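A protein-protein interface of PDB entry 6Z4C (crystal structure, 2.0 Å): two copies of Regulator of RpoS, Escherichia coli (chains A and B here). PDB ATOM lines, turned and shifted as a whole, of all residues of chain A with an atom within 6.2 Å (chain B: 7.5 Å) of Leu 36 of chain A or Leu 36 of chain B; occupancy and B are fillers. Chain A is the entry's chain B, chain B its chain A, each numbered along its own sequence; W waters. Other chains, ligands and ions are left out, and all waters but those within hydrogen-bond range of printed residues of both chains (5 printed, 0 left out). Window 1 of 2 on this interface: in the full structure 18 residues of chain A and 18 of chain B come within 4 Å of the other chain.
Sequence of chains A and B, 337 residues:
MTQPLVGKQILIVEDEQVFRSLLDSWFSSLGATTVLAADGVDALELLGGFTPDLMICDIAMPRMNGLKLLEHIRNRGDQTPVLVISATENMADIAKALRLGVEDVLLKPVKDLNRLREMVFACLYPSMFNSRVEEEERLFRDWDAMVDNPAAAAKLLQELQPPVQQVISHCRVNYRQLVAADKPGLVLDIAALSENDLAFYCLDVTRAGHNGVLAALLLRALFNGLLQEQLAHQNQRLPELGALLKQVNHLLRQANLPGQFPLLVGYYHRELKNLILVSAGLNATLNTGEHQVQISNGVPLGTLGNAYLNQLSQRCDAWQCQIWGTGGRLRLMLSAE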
ATOM      1  N   ILE A  10     -14.016   3.771   0.460  1.00  0.00           N
ATOM      2  CA  ILE A  10     -14.363   5.057  -0.198  1.00  0.00           C
ATOM      3  C   ILE A  10     -13.749   6.149   0.662  1.00  0.00           C
ATOM      4  O   ILE A  10     -14.098   6.183   1.843  1.00  0.00           O
ATOM      5  CB  ILE A  10     -15.897   5.258  -0.328  1.00  0.00           C
ATOM      6  CG1 ILE A  10     -16.618   4.011  -0.851  1.00  0.00           C
ATOM      7  CG2 ILE A  10     -16.243   6.522  -1.121  1.00  0.00           C
ATOM      8  CD1 ILE A  10     -16.374   3.712  -2.292  1.00  0.00           C
ATOM      9  N   LEU A  11     -12.935   7.014   0.065  1.00  0.00           N
ATOM     10  CA  LEU A  11     -12.421   8.277   0.658  1.00  0.00           C
ATOM     11  C   LEU A  11     -13.345   9.446   0.290  1.00  0.00           C
ATOM     12  O   LEU A  11     -13.596   9.697  -0.904  1.00  0.00           O
ATOM     13  CB  LEU A  11     -10.982   8.519   0.179  1.00  0.00           C
ATOM     14  CG  LEU A  11     -10.362   9.847   0.613  1.00  0.00           C
ATOM     15  CD1 LEU A  11     -10.350  10.018   2.126  1.00  0.00           C
ATOM     16  CD2 LEU A  11      -8.954  10.001   0.084  1.00  0.00           C
ATOM     17  N   ILE A  12     -13.926  10.077   1.283  1.00  0.00           N
ATOM     18  CA  ILE A  12     -14.812  11.249   1.090  1.00  0.00           C
ATOM     19  C   ILE A  12     -14.097  12.486   1.603  1.00  0.00           C
ATOM     20  O   ILE A  12     -13.828  12.530   2.809  1.00  0.00           O
ATOM     21  CB  ILE A  12     -16.149  11.023   1.815  1.00  0.00           C
ATOM     22  CG1 ILE A  12     -16.862   9.787   1.260  1.00  0.00           C
ATOM     23  CG2 ILE A  12     -17.010  12.265   1.784  1.00  0.00           C
ATOM     24  CD1 ILE A  12     -17.885   9.174   2.234  1.00  0.00           C
ATOM     25  N   VAL A  13     -13.856  13.466   0.736  1.00  0.00           N
ATOM     26  CA  VAL A  13     -13.200  14.744   1.127  1.00  0.00           C
ATOM     27  C   VAL A  13     -14.260  15.861   1.041  1.00  0.00           C
ATOM     28  O   VAL A  13     -14.722  16.153  -0.092  1.00  0.00           O
ATOM     29  CB  VAL A  13     -11.958  15.045   0.267  1.00  0.00           C
ATOM     30  CG1 VAL A  13     -11.216  16.258   0.813  1.00  0.00           C
ATOM     31  CG2 VAL A  13     -11.009  13.876   0.148  1.00  0.00           C
ATOM     32  N   ARG A  20     -20.975  15.889   4.852  1.00  0.00           N
ATOM     33  CA  ARG A  20     -19.965  14.848   5.147  1.00  0.00           C
ATOM     34  C   ARG A  20     -20.673  13.662   5.811  1.00  0.00           C
ATOM     35  O   ARG A  20     -20.432  12.518   5.382  1.00  0.00           O
ATOM     36  CB  ARG A  20     -18.856  15.488   5.965  1.00  0.00           C
ATOM     37  CG  ARG A  20     -17.712  14.561   6.313  1.00  0.00           C
ATOM     38  CD  ARG A  20     -16.474  15.323   6.683  1.00  0.00           C
ATOM     39  NE  ARG A  20     -16.542  15.970   7.983  1.00  0.00           N
ATOM     40  CZ  ARG A  20     -16.436  17.269   8.220  1.00  0.00           C
ATOM     41  NH1 ARG A  20     -16.344  18.132   7.222  1.00  0.00           N
ATOM     42  NH2 ARG A  20     -16.451  17.713   9.466  1.00  0.00           N
ATOM     43  N   SER A  21     -21.556  13.935   6.774  1.00  0.00           N
ATOM     44  CA  SER A  21     -22.351  12.930   7.520  1.00  0.00           C
ATOM     45  C   SER A  21     -23.315  12.225   6.585  1.00  0.00           C
ATOM     46  O   SER A  21     -23.440  10.985   6.713  1.00  0.00           O
ATOM     47  CB  SER A  21     -23.094  13.546   8.658  1.00  0.00           C
ATOM     48  OG  SER A  21     -22.200  14.251   9.503  1.00  0.00           O
ATOM     49  N   LEU A  23     -23.071  11.798   3.349  1.00  0.00           N
ATOM     50  CA  LEU A  23     -22.285  10.941   2.426  1.00  0.00           C
ATOM     51  C   LEU A  23     -21.775   9.729   3.201  1.00  0.00           C
ATOM     52  O   LEU A  23     -21.739   8.652   2.603  1.00  0.00           O
ATOM     53  CB  LEU A  23     -21.134  11.735   1.815  1.00  0.00           C
ATOM     54  CG  LEU A  23     -21.540  12.671   0.677  1.00  0.00           C
ATOM     55  CD1 LEU A  23     -20.343  13.470   0.177  1.00  0.00           C
ATOM     56  CD2 LEU A  23     -22.153  11.891  -0.472  1.00  0.00           C
ATOM     57  N   ASP A  24     -21.373   9.899   4.468  1.00  0.00           N
ATOM     58  CA  ASP A  24     -20.882   8.748   5.285  1.00  0.00           C
ATOM     59  C   ASP A  24     -22.053   7.765   5.460  1.00  0.00           C
ATOM     60  O   ASP A  24     -21.934   6.562   5.066  1.00  0.00           O
ATOM     61  CB  ASP A  24     -20.291   9.201   6.625  1.00  0.00           C
ATOM     62  CG  ASP A  24     -19.679   8.060   7.417  1.00  0.00           C
ATOM     63  OD1 ASP A  24     -19.432   6.997   6.813  1.00  0.00           O
ATOM     64  OD2 ASP A  24     -19.380   8.264   8.600  1.00  0.00           O
ATOM     65  N   THR A  34     -15.778   3.599   4.937  1.00  0.00           N
ATOM     66  CA  THR A  34     -15.506   5.008   4.644  1.00  0.00           C
ATOM     67  C   THR A  34     -14.310   5.523   5.448  1.00  0.00           C
ATOM     68  O   THR A  34     -14.054   5.066   6.562  1.00  0.00           O
ATOM     69  CB  THR A  34     -16.769   5.836   4.785  1.00  0.00           C
ATOM     70  OG1 THR A  34     -17.206   5.721   6.135  1.00  0.00           O
ATOM     71  CG2 THR A  34     -17.826   5.374   3.797  1.00  0.00           C
ATOM     72  N   VAL A  35     -13.550   6.370   4.776  1.00  0.00           N
ATOM     73  CA  VAL A  35     -12.626   7.330   5.396  1.00  0.00           C
ATOM     74  C   VAL A  35     -13.091   8.709   4.972  1.00  0.00           C
ATOM     75  O   VAL A  35     -13.307   8.908   3.804  1.00  0.00           O
ATOM     76  CB  VAL A  35     -11.185   7.051   4.969  1.00  0.00           C
ATOM     77  CG1 VAL A  35     -10.263   8.085   5.556  1.00  0.00           C
ATOM     78  CG2 VAL A  35     -10.766   5.647   5.337  1.00  0.00           C
ATOM     79  N   LEU A  36     -13.266   9.608   5.928  1.00  0.00           N
ATOM     80  CA  LEU A  36     -13.746  10.989   5.701  1.00  0.00           C
ATOM     81  C   LEU A  36     -12.629  11.948   6.103  1.00  0.00           C
ATOM     82  O   LEU A  36     -11.957  11.770   7.155  1.00  0.00           O
ATOM     83  CB  LEU A  36     -14.993  11.221   6.550  1.00  0.00           C
ATOM     84  CG  LEU A  36     -16.073  10.146   6.444  1.00  0.00           C
ATOM     85  CD1 LEU A  36     -16.991  10.217   7.642  1.00  0.00           C
ATOM     86  CD2 LEU A  36     -16.885  10.340   5.195  1.00  0.00           C
ATOM     87  N   ALA A  37     -12.437  12.978   5.322  1.00  0.00           N
ATOM     88  CA  ALA A  37     -11.439  13.997   5.646  1.00  0.00           C
ATOM     89  C   ALA A  37     -12.116  15.352   5.471  1.00  0.00           C
ATOM     90  O   ALA A  37     -12.684  15.618   4.382  1.00  0.00           O
ATOM     91  CB  ALA A  37     -10.239  13.776   4.772  1.00  0.00           C
ATOM     92  N   ALA A  38     -12.066  16.184   6.506  1.00  0.00           N
ATOM     93  CA  ALA A  38     -12.693  17.528   6.510  1.00  0.00           C
ATOM     94  C   ALA A  38     -11.889  18.475   5.601  1.00  0.00           C
ATOM     95  O   ALA A  38     -12.450  19.417   4.989  1.00  0.00           O
ATOM     96  CB  ALA A  38     -12.796  17.989   7.940  1.00  0.00           C
ATOM     97  N   LEU A  46      -3.063  11.698   3.571  1.00  0.00           N
ATOM     98  CA  LEU A  46      -3.543  10.310   3.778  1.00  0.00           C
ATOM     99  C   LEU A  46      -3.187   9.454   2.571  1.00  0.00           C
ATOM    100  O   LEU A  46      -2.944   8.264   2.745  1.00  0.00           O
ATOM    101  CB  LEU A  46      -5.068  10.270   3.956  1.00  0.00           C
ATOM    102  CG  LEU A  46      -5.616  10.992   5.163  1.00  0.00           C
ATOM    103  CD1 LEU A  46      -7.124  10.969   5.132  1.00  0.00           C
ATOM    104  CD2 LEU A  46      -5.084  10.361   6.435  1.00  0.00           C
ATOM    105  N   ILE B  10      -7.436  15.504  14.304  1.00  0.00           N
ATOM    106  CA  ILE B  10      -7.982  14.421  15.171  1.00  0.00           C
ATOM    107  C   ILE B  10      -8.359  13.268  14.238  1.00  0.00           C
ATOM    108  O   ILE B  10      -9.131  13.502  13.281  1.00  0.00           O
ATOM    109  CB  ILE B  10      -9.215  14.849  15.996  1.00  0.00           C
ATOM    110  CG1 ILE B  10      -9.081  16.221  16.669  1.00  0.00           C
ATOM    111  CG2 ILE B  10      -9.611  13.760  16.994  1.00  0.00           C
ATOM    112  CD1 ILE B  10      -8.092  16.282  17.777  1.00  0.00           C
ATOM    113  N   LEU B  11      -7.913  12.069  14.559  1.00  0.00           N
ATOM    114  CA  LEU B  11      -8.325  10.817  13.873  1.00  0.00           C
ATOM    115  C   LEU B  11      -9.362  10.092  14.734  1.00  0.00           C
ATOM    116  O   LEU B  11      -9.088   9.793  15.917  1.00  0.00           O
ATOM    117  CB  LEU B  11      -7.104   9.942  13.612  1.00  0.00           C
ATOM    118  CG  LEU B  11      -7.417   8.519  13.140  1.00  0.00           C
ATOM    119  CD1 LEU B  11      -8.202   8.534  11.837  1.00  0.00           C
ATOM    120  CD2 LEU B  11      -6.143   7.764  12.953  1.00  0.00           C
ATOM    121  N   ILE B  12     -10.539   9.893  14.199  1.00  0.00           N
ATOM    122  CA  ILE B  12     -11.640   9.221  14.950  1.00  0.00           C
ATOM    123  C   ILE B  12     -11.878   7.857  14.334  1.00  0.00           C
ATOM    124  O   ILE B  12     -12.216   7.824  13.166  1.00  0.00           O
ATOM    125  CB  ILE B  12     -12.892  10.089  14.940  1.00  0.00           C
ATOM    126  CG1 ILE B  12     -12.592  11.450  15.572  1.00  0.00           C
ATOM    127  CG2 ILE B  12     -14.064   9.359  15.598  1.00  0.00           C
ATOM    128  CD1 ILE B  12     -13.582  12.536  15.164  1.00  0.00           C
ATOM    129  N   VAL B  13     -11.681   6.785  15.094  1.00  0.00           N
ATOM    130  CA  VAL B  13     -11.908   5.405  14.590  1.00  0.00           C
ATOM    131  C   VAL B  13     -13.150   4.838  15.300  1.00  0.00           C
ATOM    132  O   VAL B  13     -13.110   4.662  16.534  1.00  0.00           O
ATOM    133  CB  VAL B  13     -10.653   4.529  14.775  1.00  0.00           C
ATOM    134  CG1 VAL B  13     -10.829   3.161  14.106  1.00  0.00           C
ATOM    135  CG2 VAL B  13      -9.399   5.202  14.271  1.00  0.00           C
ATOM    136  N   GLU B  14     -14.237   4.633  14.561  1.00  0.00           N
ATOM    137  CA  GLU B  14     -15.571   4.396  15.153  1.00  0.00           C
ATOM    138  C   GLU B  14     -16.464   3.666  14.154  1.00  0.00           C
ATOM    139  O   GLU B  14     -16.798   4.238  13.094  1.00  0.00           O
ATOM    140  CB  GLU B  14     -16.212   5.699  15.614  1.00  0.00           C
ATOM    141  CG  GLU B  14     -17.622   5.522  16.175  1.00  0.00           C
ATOM    142  CD  GLU B  14     -17.763   4.406  17.215  1.00  0.00           C
ATOM    143  OE1 GLU B  14     -17.040   4.453  18.213  1.00  0.00           O
ATOM    144  OE2 GLU B  14     -18.563   3.463  16.990  1.00  0.00           O
ATOM    145  N   GLN B  17     -21.920   4.524  12.627  1.00  0.00           N
ATOM    146  CA  GLN B  17     -22.186   5.753  11.815  1.00  0.00           C
ATOM    147  C   GLN B  17     -22.664   6.922  12.693  1.00  0.00           C
ATOM    148  O   GLN B  17     -22.135   8.013  12.521  1.00  0.00           O
ATOM    149  CB  GLN B  17     -23.198   5.429  10.708  1.00  0.00           C
ATOM    150  CG  GLN B  17     -24.224   6.524  10.419  1.00  0.00           C
ATOM    151  CD  GLN B  17     -23.545   7.799  10.003  1.00  0.00           C
ATOM    152  OE1 GLN B  17     -22.525   7.777   9.317  1.00  0.00           O
ATOM    153  NE2 GLN B  17     -24.099   8.917  10.433  1.00  0.00           N
ATOM    154  N   PHE B  19     -22.586   7.517  16.054  1.00  0.00           N
ATOM    155  CA  PHE B  19     -21.577   7.971  17.047  1.00  0.00           C
ATOM    156  C   PHE B  19     -20.439   8.650  16.266  1.00  0.00           C
ATOM    157  O   PHE B  19     -19.900   9.675  16.716  1.00  0.00           O
ATOM    158  CB  PHE B  19     -21.137   6.830  17.980  1.00  0.00           C
ATOM    159  CG  PHE B  19     -20.419   7.298  19.216  1.00  0.00           C
ATOM    160  CD1 PHE B  19     -20.950   8.303  20.007  1.00  0.00           C
ATOM    161  CD2 PHE B  19     -19.165   6.810  19.532  1.00  0.00           C
ATOM    162  CE1 PHE B  19     -20.253   8.800  21.099  1.00  0.00           C
ATOM    163  CE2 PHE B  19     -18.461   7.305  20.621  1.00  0.00           C
ATOM    164  CZ  PHE B  19     -19.012   8.289  21.413  1.00  0.00           C
ATOM    165  N   ARG B  20     -20.112   8.109  15.094  1.00  0.00           N
ATOM    166  CA  ARG B  20     -19.027   8.639  14.236  1.00  0.00           C
ATOM    167  C   ARG B  20     -19.359  10.105  13.913  1.00  0.00           C
ATOM    168  O   ARG B  20     -18.473  10.979  14.106  1.00  0.00           O
ATOM    169  CB  ARG B  20     -18.898   7.740  13.005  1.00  0.00           C
ATOM    170  CG  ARG B  20     -17.748   8.090  12.080  1.00  0.00           C
ATOM    171  CD  ARG B  20     -17.298   6.932  11.225  1.00  0.00           C
ATOM    172  NE  ARG B  20     -18.280   6.517  10.242  1.00  0.00           N
ATOM    173  CZ  ARG B  20     -18.877   5.336  10.177  1.00  0.00           C
ATOM    174  NH1 ARG B  20     -18.637   4.420  11.096  1.00  0.00           N
ATOM    175  NH2 ARG B  20     -19.716   5.074   9.180  1.00  0.00           N
ATOM    176  N   SER B  21     -20.607  10.350  13.497  1.00  0.00           N
ATOM    177  CA  SER B  21     -21.162  11.658  13.084  1.00  0.00           C
ATOM    178  C   SER B  21     -21.222  12.615  14.267  1.00  0.00           C
ATOM    179  O   SER B  21     -20.908  13.792  14.056  1.00  0.00           O
ATOM    180  CB  SER B  21     -22.518  11.510  12.459  1.00  0.00           C
ATOM    181  OG  SER B  21     -22.472  10.608  11.360  1.00  0.00           O
ATOM    182  N   LEU B  23     -19.262  12.531  16.948  1.00  0.00           N
ATOM    183  CA  LEU B  23     -17.872  12.885  17.321  1.00  0.00           C
ATOM    184  C   LEU B  23     -17.335  13.858  16.269  1.00  0.00           C
ATOM    185  O   LEU B  23     -16.623  14.783  16.651  1.00  0.00           O
ATOM    186  CB  LEU B  23     -17.030  11.621  17.400  1.00  0.00           C
ATOM    187  CG  LEU B  23     -17.170  10.798  18.685  1.00  0.00           C
ATOM    188  CD1 LEU B  23     -16.388   9.494  18.538  1.00  0.00           C
ATOM    189  CD2 LEU B  23     -16.680  11.557  19.917  1.00  0.00           C
ATOM    190  N   ASP B  24     -17.678  13.644  14.990  1.00  0.00           N
ATOM    191  CA  ASP B  24     -17.213  14.518  13.871  1.00  0.00           C
ATOM    192  C   ASP B  24     -17.762  15.921  14.153  1.00  0.00           C
ATOM    193  O   ASP B  24     -16.965  16.893  14.149  1.00  0.00           O
ATOM    194  CB  ASP B  24     -17.610  13.973  12.494  1.00  0.00           C
ATOM    195  CG  ASP B  24     -16.998  14.729  11.323  1.00  0.00           C
ATOM    196  OD1 ASP B  24     -16.047  15.470  11.555  1.00  0.00           O
ATOM    197  OD2 ASP B  24     -17.449  14.516  10.166  1.00  0.00           O
ATOM    198  N   SER B  25     -19.067  15.977  14.448  1.00  0.00           N
ATOM    199  CA  SER B  25     -19.843  17.203  14.749  1.00  0.00           C
ATOM    200  C   SER B  25     -19.209  17.980  15.891  1.00  0.00           C
ATOM    201  O   SER B  25     -18.931  19.200  15.752  1.00  0.00           O
ATOM    202  CB  SER B  25     -21.259  16.861  15.075  1.00  0.00           C
ATOM    203  OG  SER B  25     -22.007  18.059  15.083  1.00  0.00           O
ATOM    204  N   PHE B  27     -16.076  17.617  17.532  1.00  0.00           N
ATOM    205  CA  PHE B  27     -14.672  18.037  17.302  1.00  0.00           C
ATOM    206  C   PHE B  27     -14.605  19.147  16.256  1.00  0.00           C
ATOM    207  O   PHE B  27     -13.738  20.054  16.413  1.00  0.00           O
ATOM    208  CB  PHE B  27     -13.784  16.844  16.926  1.00  0.00           C
ATOM    209  CG  PHE B  27     -13.295  16.056  18.112  1.00  0.00           C
ATOM    210  CD1 PHE B  27     -12.221  16.501  18.855  1.00  0.00           C
ATOM    211  CD2 PHE B  27     -13.887  14.850  18.452  1.00  0.00           C
ATOM    212  CE1 PHE B  27     -11.774  15.776  19.947  1.00  0.00           C
ATOM    213  CE2 PHE B  27     -13.455  14.138  19.555  1.00  0.00           C
ATOM    214  CZ  PHE B  27     -12.396  14.602  20.305  1.00  0.00           C
ATOM    215  N   SER B  28     -15.373  19.022  15.177  1.00  0.00           N
ATOM    216  CA  SER B  28     -15.463  20.022  14.086  1.00  0.00           C
ATOM    217  C   SER B  28     -16.001  21.350  14.657  1.00  0.00           C
ATOM    218  O   SER B  28     -15.387  22.389  14.426  1.00  0.00           O
ATOM    219  CB  SER B  28     -16.300  19.493  12.962  1.00  0.00           C
ATOM    220  OG  SER B  28     -15.573  18.501  12.253  1.00  0.00           O
ATOM    221  N   THR B  34     -10.897  16.921  11.238  1.00  0.00           N
ATOM    222  CA  THR B  34     -11.133  15.503  11.518  1.00  0.00           C
ATOM    223  C   THR B  34     -10.790  14.622  10.303  1.00  0.00           C
ATOM    224  O   THR B  34     -10.975  15.027   9.154  1.00  0.00           O
ATOM    225  CB  THR B  34     -12.557  15.284  12.022  1.00  0.00           C
ATOM    226  OG1 THR B  34     -13.487  15.768  11.058  1.00  0.00           O
ATOM    227  CG2 THR B  34     -12.785  15.995  13.343  1.00  0.00           C
ATOM    228  N   VAL B  35     -10.280  13.439  10.622  1.00  0.00           N
ATOM    229  CA  VAL B  35     -10.280  12.248   9.771  1.00  0.00           C
ATOM    230  C   VAL B  35     -11.036  11.156  10.520  1.00  0.00           C
ATOM    231  O   VAL B  35     -10.711  10.865  11.677  1.00  0.00           O
ATOM    232  CB  VAL B  35      -8.848  11.840   9.417  1.00  0.00           C
ATOM    233  CG1 VAL B  35      -8.876  10.618   8.544  1.00  0.00           C
ATOM    234  CG2 VAL B  35      -8.076  12.962   8.752  1.00  0.00           C
ATOM    235  N   LEU B  36     -12.032  10.577   9.874  1.00  0.00           N
ATOM    236  CA  LEU B  36     -12.865   9.498  10.444  1.00  0.00           C
ATOM    237  C   LEU B  36     -12.599   8.203   9.669  1.00  0.00           C
ATOM    238  O   LEU B  36     -12.533   8.215   8.423  1.00  0.00           O
ATOM    239  CB  LEU B  36     -14.341   9.892  10.345  1.00  0.00           C
ATOM    240  CG  LEU B  36     -14.702  11.339  10.701  1.00  0.00           C
ATOM    241  CD1 LEU B  36     -16.110  11.637  10.222  1.00  0.00           C
ATOM    242  CD2 LEU B  36     -14.660  11.557  12.175  1.00  0.00           C
ATOM    243  N   ALA B  37     -12.485   7.100  10.370  1.00  0.00           N
ATOM    244  CA  ALA B  37     -12.379   5.781   9.733  1.00  0.00           C
ATOM    245  C   ALA B  37     -13.419   4.848  10.369  1.00  0.00           C
ATOM    246  O   ALA B  37     -13.438   4.714  11.621  1.00  0.00           O
ATOM    247  CB  ALA B  37     -10.961   5.295   9.878  1.00  0.00           C
ATOM    248  N   ALA B  38     -14.268   4.232   9.544  1.00  0.00           N
ATOM    249  CA  ALA B  38     -15.293   3.252   9.977  1.00  0.00           C
ATOM    250  C   ALA B  38     -14.613   2.000  10.561  1.00  0.00           C
ATOM    251  O   ALA B  38     -15.156   1.328  11.480  1.00  0.00           O
ATOM    252  CB  ALA B  38     -16.202   2.943   8.797  1.00  0.00           C
ATOM    253  N   ASP B  39     -13.394   1.720  10.116  1.00  0.00           N
ATOM    254  CA  ASP B  39     -12.773   0.388  10.222  1.00  0.00           C
ATOM    255  C   ASP B  39     -11.347   0.532  10.768  1.00  0.00           C
ATOM    256  O   ASP B  39     -10.578   1.342  10.222  1.00  0.00           O
ATOM    257  CB  ASP B  39     -12.825  -0.261   8.826  1.00  0.00           C
ATOM    258  CG  ASP B  39     -12.245  -1.659   8.802  1.00  0.00           C
ATOM    259  OD1 ASP B  39     -13.033  -2.619   8.870  1.00  0.00           O
ATOM    260  OD2 ASP B  39     -11.004  -1.771   8.755  1.00  0.00           O
ATOM    261  N   ASP B  42      -8.328  -0.112   8.337  1.00  0.00           N
ATOM    262  CA  ASP B  42      -8.127   1.076   7.469  1.00  0.00           C
ATOM    263  C   ASP B  42      -7.366   2.170   8.249  1.00  0.00           C
ATOM    264  O   ASP B  42      -6.454   2.776   7.659  1.00  0.00           O
ATOM    265  CB  ASP B  42      -9.443   1.615   6.945  1.00  0.00           C
ATOM    266  CG  ASP B  42     -10.199   0.781   5.915  1.00  0.00           C
ATOM    267  OD1 ASP B  42      -9.686  -0.252   5.455  1.00  0.00           O
ATOM    268  OD2 ASP B  42     -11.316   1.213   5.556  1.00  0.00           O
ATOM    269  N   ALA B  43      -7.698   2.402   9.527  1.00  0.00           N
ATOM    270  CA  ALA B  43      -6.967   3.362  10.399  1.00  0.00           C
ATOM    271  C   ALA B  43      -5.484   2.935  10.537  1.00  0.00           C
ATOM    272  O   ALA B  43      -4.589   3.777  10.416  1.00  0.00           O
ATOM    273  CB  ALA B  43      -7.655   3.436  11.732  1.00  0.00           C
ATOM    274  N   LEU B  46      -3.960   3.980   7.255  1.00  0.00           N
ATOM    275  CA  LEU B  46      -3.845   5.463   7.211  1.00  0.00           C
ATOM    276  C   LEU B  46      -2.660   5.925   8.031  1.00  0.00           C
ATOM    277  O   LEU B  46      -2.001   6.895   7.621  1.00  0.00           O
ATOM    278  CB  LEU B  46      -5.080   6.139   7.807  1.00  0.00           C
ATOM    279  CG  LEU B  46      -6.375   5.927   7.069  1.00  0.00           C
ATOM    280  CD1 LEU B  46      -7.507   6.586   7.840  1.00  0.00           C
ATOM    281  CD2 LEU B  46      -6.249   6.455   5.659  1.00  0.00           C
HETATM  282  O   HOH W   1      -9.197  16.479   7.418  1.00  0.00           O
HETATM  283  O   HOH W   2     -12.504   2.823   7.393  1.00  0.00           O
HETATM  284  O   HOH W   3      -1.517   7.469   4.913  1.00  0.00           O
HETATM  285  O   HOH W   4     -19.715  13.040   9.775  1.00  0.00           O
HETATM  286  O   HOH W   5     -20.140  10.579   9.904  1.00  0.00           O
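Water W3 lies within hydrogen-bond range of the backbone carbonyl oxygen (O) of Leu 46 of chain A (2.7 Å) and the backbone carbonyl oxygen (O) of Leu 46 of chain B (2.8 Å). Water W4 lies within hydrogen-bond range of OD2 of Asp 24 of chain B (2.7 Å) and OG of Ser 21 of chain A (2.8 Å). Water W5 bridges OG of Ser 21 of chain B and OD2 of Asp 24 of chain A. Water W1 bridges O of Thr 34 of chain B (2.9 Å) and N of Ala 38 of chain A (3.0 Å).
Hydrophobic or aromatic side chains of chain A that line the printed part of chain B: Val 35, Leu 36, Ala 38 and Leu 46. Of the 23 printed residues of chain B, 10 touch a printed residue of chain A. Hydrophobic or aromatic side chains of chain B that line the printed part of chain A: Val 35, Leu 36, Ala 38 and Leu 46. Among the printed residues, 17 pairs touch across the chains.
Of chain B, only Thr 34, Val 35 and Leu 36 come within 4 Å of Leu 36 of chain A. Of chain A, only Thr 34 (3.96 Å), Val 35 (3.2 Å) and Leu 36 (3.0 Å) come within 4 Å of Leu 36 of chain B. Printed residues of chain B within 4 Å of Val 35 of chain A: Leu 36 and Leu 46. Of the printed residues of chain B, Ala 37 of chain A touches Thr 34 (3.7 Å). Printed residues of chain B within 4 Å of Asp 24 of chain A: Gln 17 (3.3 Å) and Arg 20 (2.6 Å). Asp 42 of chain B touches none of the printed residues of chain A. Ile 12 of chain A touches none of the printed residues of chain B. The nearest residue of chain B that does not touch Leu 36 of chain A is Arg 20 of chain B (4.7 Å). The nearest residue of chain A that does not touch Leu 36 of chain B is Arg 20 of chain A (4.9 Å). The nearest printed residue of chain A that does not touch Asp 24 of chain B is Ser 21 of chain A (4.8 Å).
N of Ile 12 of chain B is in hydrogen-bond range of O of Val 35 of chain B. N of Val 35 of chain A lies within hydrogen-bond range of O of Ile 10 of chain A (3.0 Å). The backbone NH (N) of Ile 12 of chain A sits at hydrogen-bond distance from the backbone carbonyl oxygen (O) of Val 35 of chain A (2.8 Å). The side-chain carboxylate of Asp 24 of chain A sits at hydrogen-bond distance from the side-chain hydroxyl of Thr 34 of chain A, at 2.7 Å.
OE1 of Gln 17 of chain B lies close to OD2 of Asp 24 of chain A, 3.3 Å away. The guanidinium group of Arg 20 of chain B is in salt-bridge range of the side-chain carboxylate of Asp 24 of chain A, 2.6 Å away. The guanidinium group of Arg 20 of chain A is in salt-bridge range of the side-chain carboxylate of Asp 24 of chain B. The side-chain hydroxyl of Ser 28 of chain B sits at hydrogen-bond distance from the guanidinium group of Arg 20 of chain A, 3.0 Å away. The backbone carbonyl oxygen (O) of Thr 34 of chain B lies within hydrogen-bond range of the backbone NH (N) of Ala 38 of chain A. The backbone carbonyl oxygen (O) of Leu 36 of chain B is in hydrogen-bond range of the backbone NH (N) of Leu 36 of chain A (3.0 Å). The backbone carbonyl oxygen (O) of Thr 34 of chain A lies within hydrogen-bond range of the backbone NH (N) of Ala 38 of chain B, at 3.1 Å.
Among the printed residues, merely in contact across the chains: Arg 20 of chain A with Thr 34 of chain B (3.9 Å), Thr 34 of chain A with Arg 20 of chain B (3.999 Å), Thr 34 of chain A with Leu 36 of chain B (3.96 Å), Thr 34 of chain A with Ala 37 of chain B (3.7 Å), Val 35 of chain A with Leu 36 of chain B (3.2 Å), Val 35 of chain A with Leu 46 of chain B (3.9 Å), Leu 36 of chain A with Thr 34 of chain B (3.9 Å), Leu 36 of chain A with Val 35 of chain B (3.1 Å), Ala 37 of chain A with Thr 34 of chain B (3.7 Å) and Leu 46 of chain A with Val 35 of chain B (3.9 Å).
Arg 20 of chain A touches Thr 34 of chain B, and with the chains exchanged Thr 34 of chain A touches Arg 20 of chain B. Thr 34 of chain A touches Ala 37 of chain B, and with the chains exchanged Ala 37 of chain A touches Thr 34 of chain B. Val 35 of chain A touches Leu 36 of chain B, and with the chains exchanged Leu 36 of chain A touches Val 35 of chain B. Positions printed for both chains: 10, 11, 12, 13, 20, 21, 23, 24, 34, 35, 36, 37, 38 and 46.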
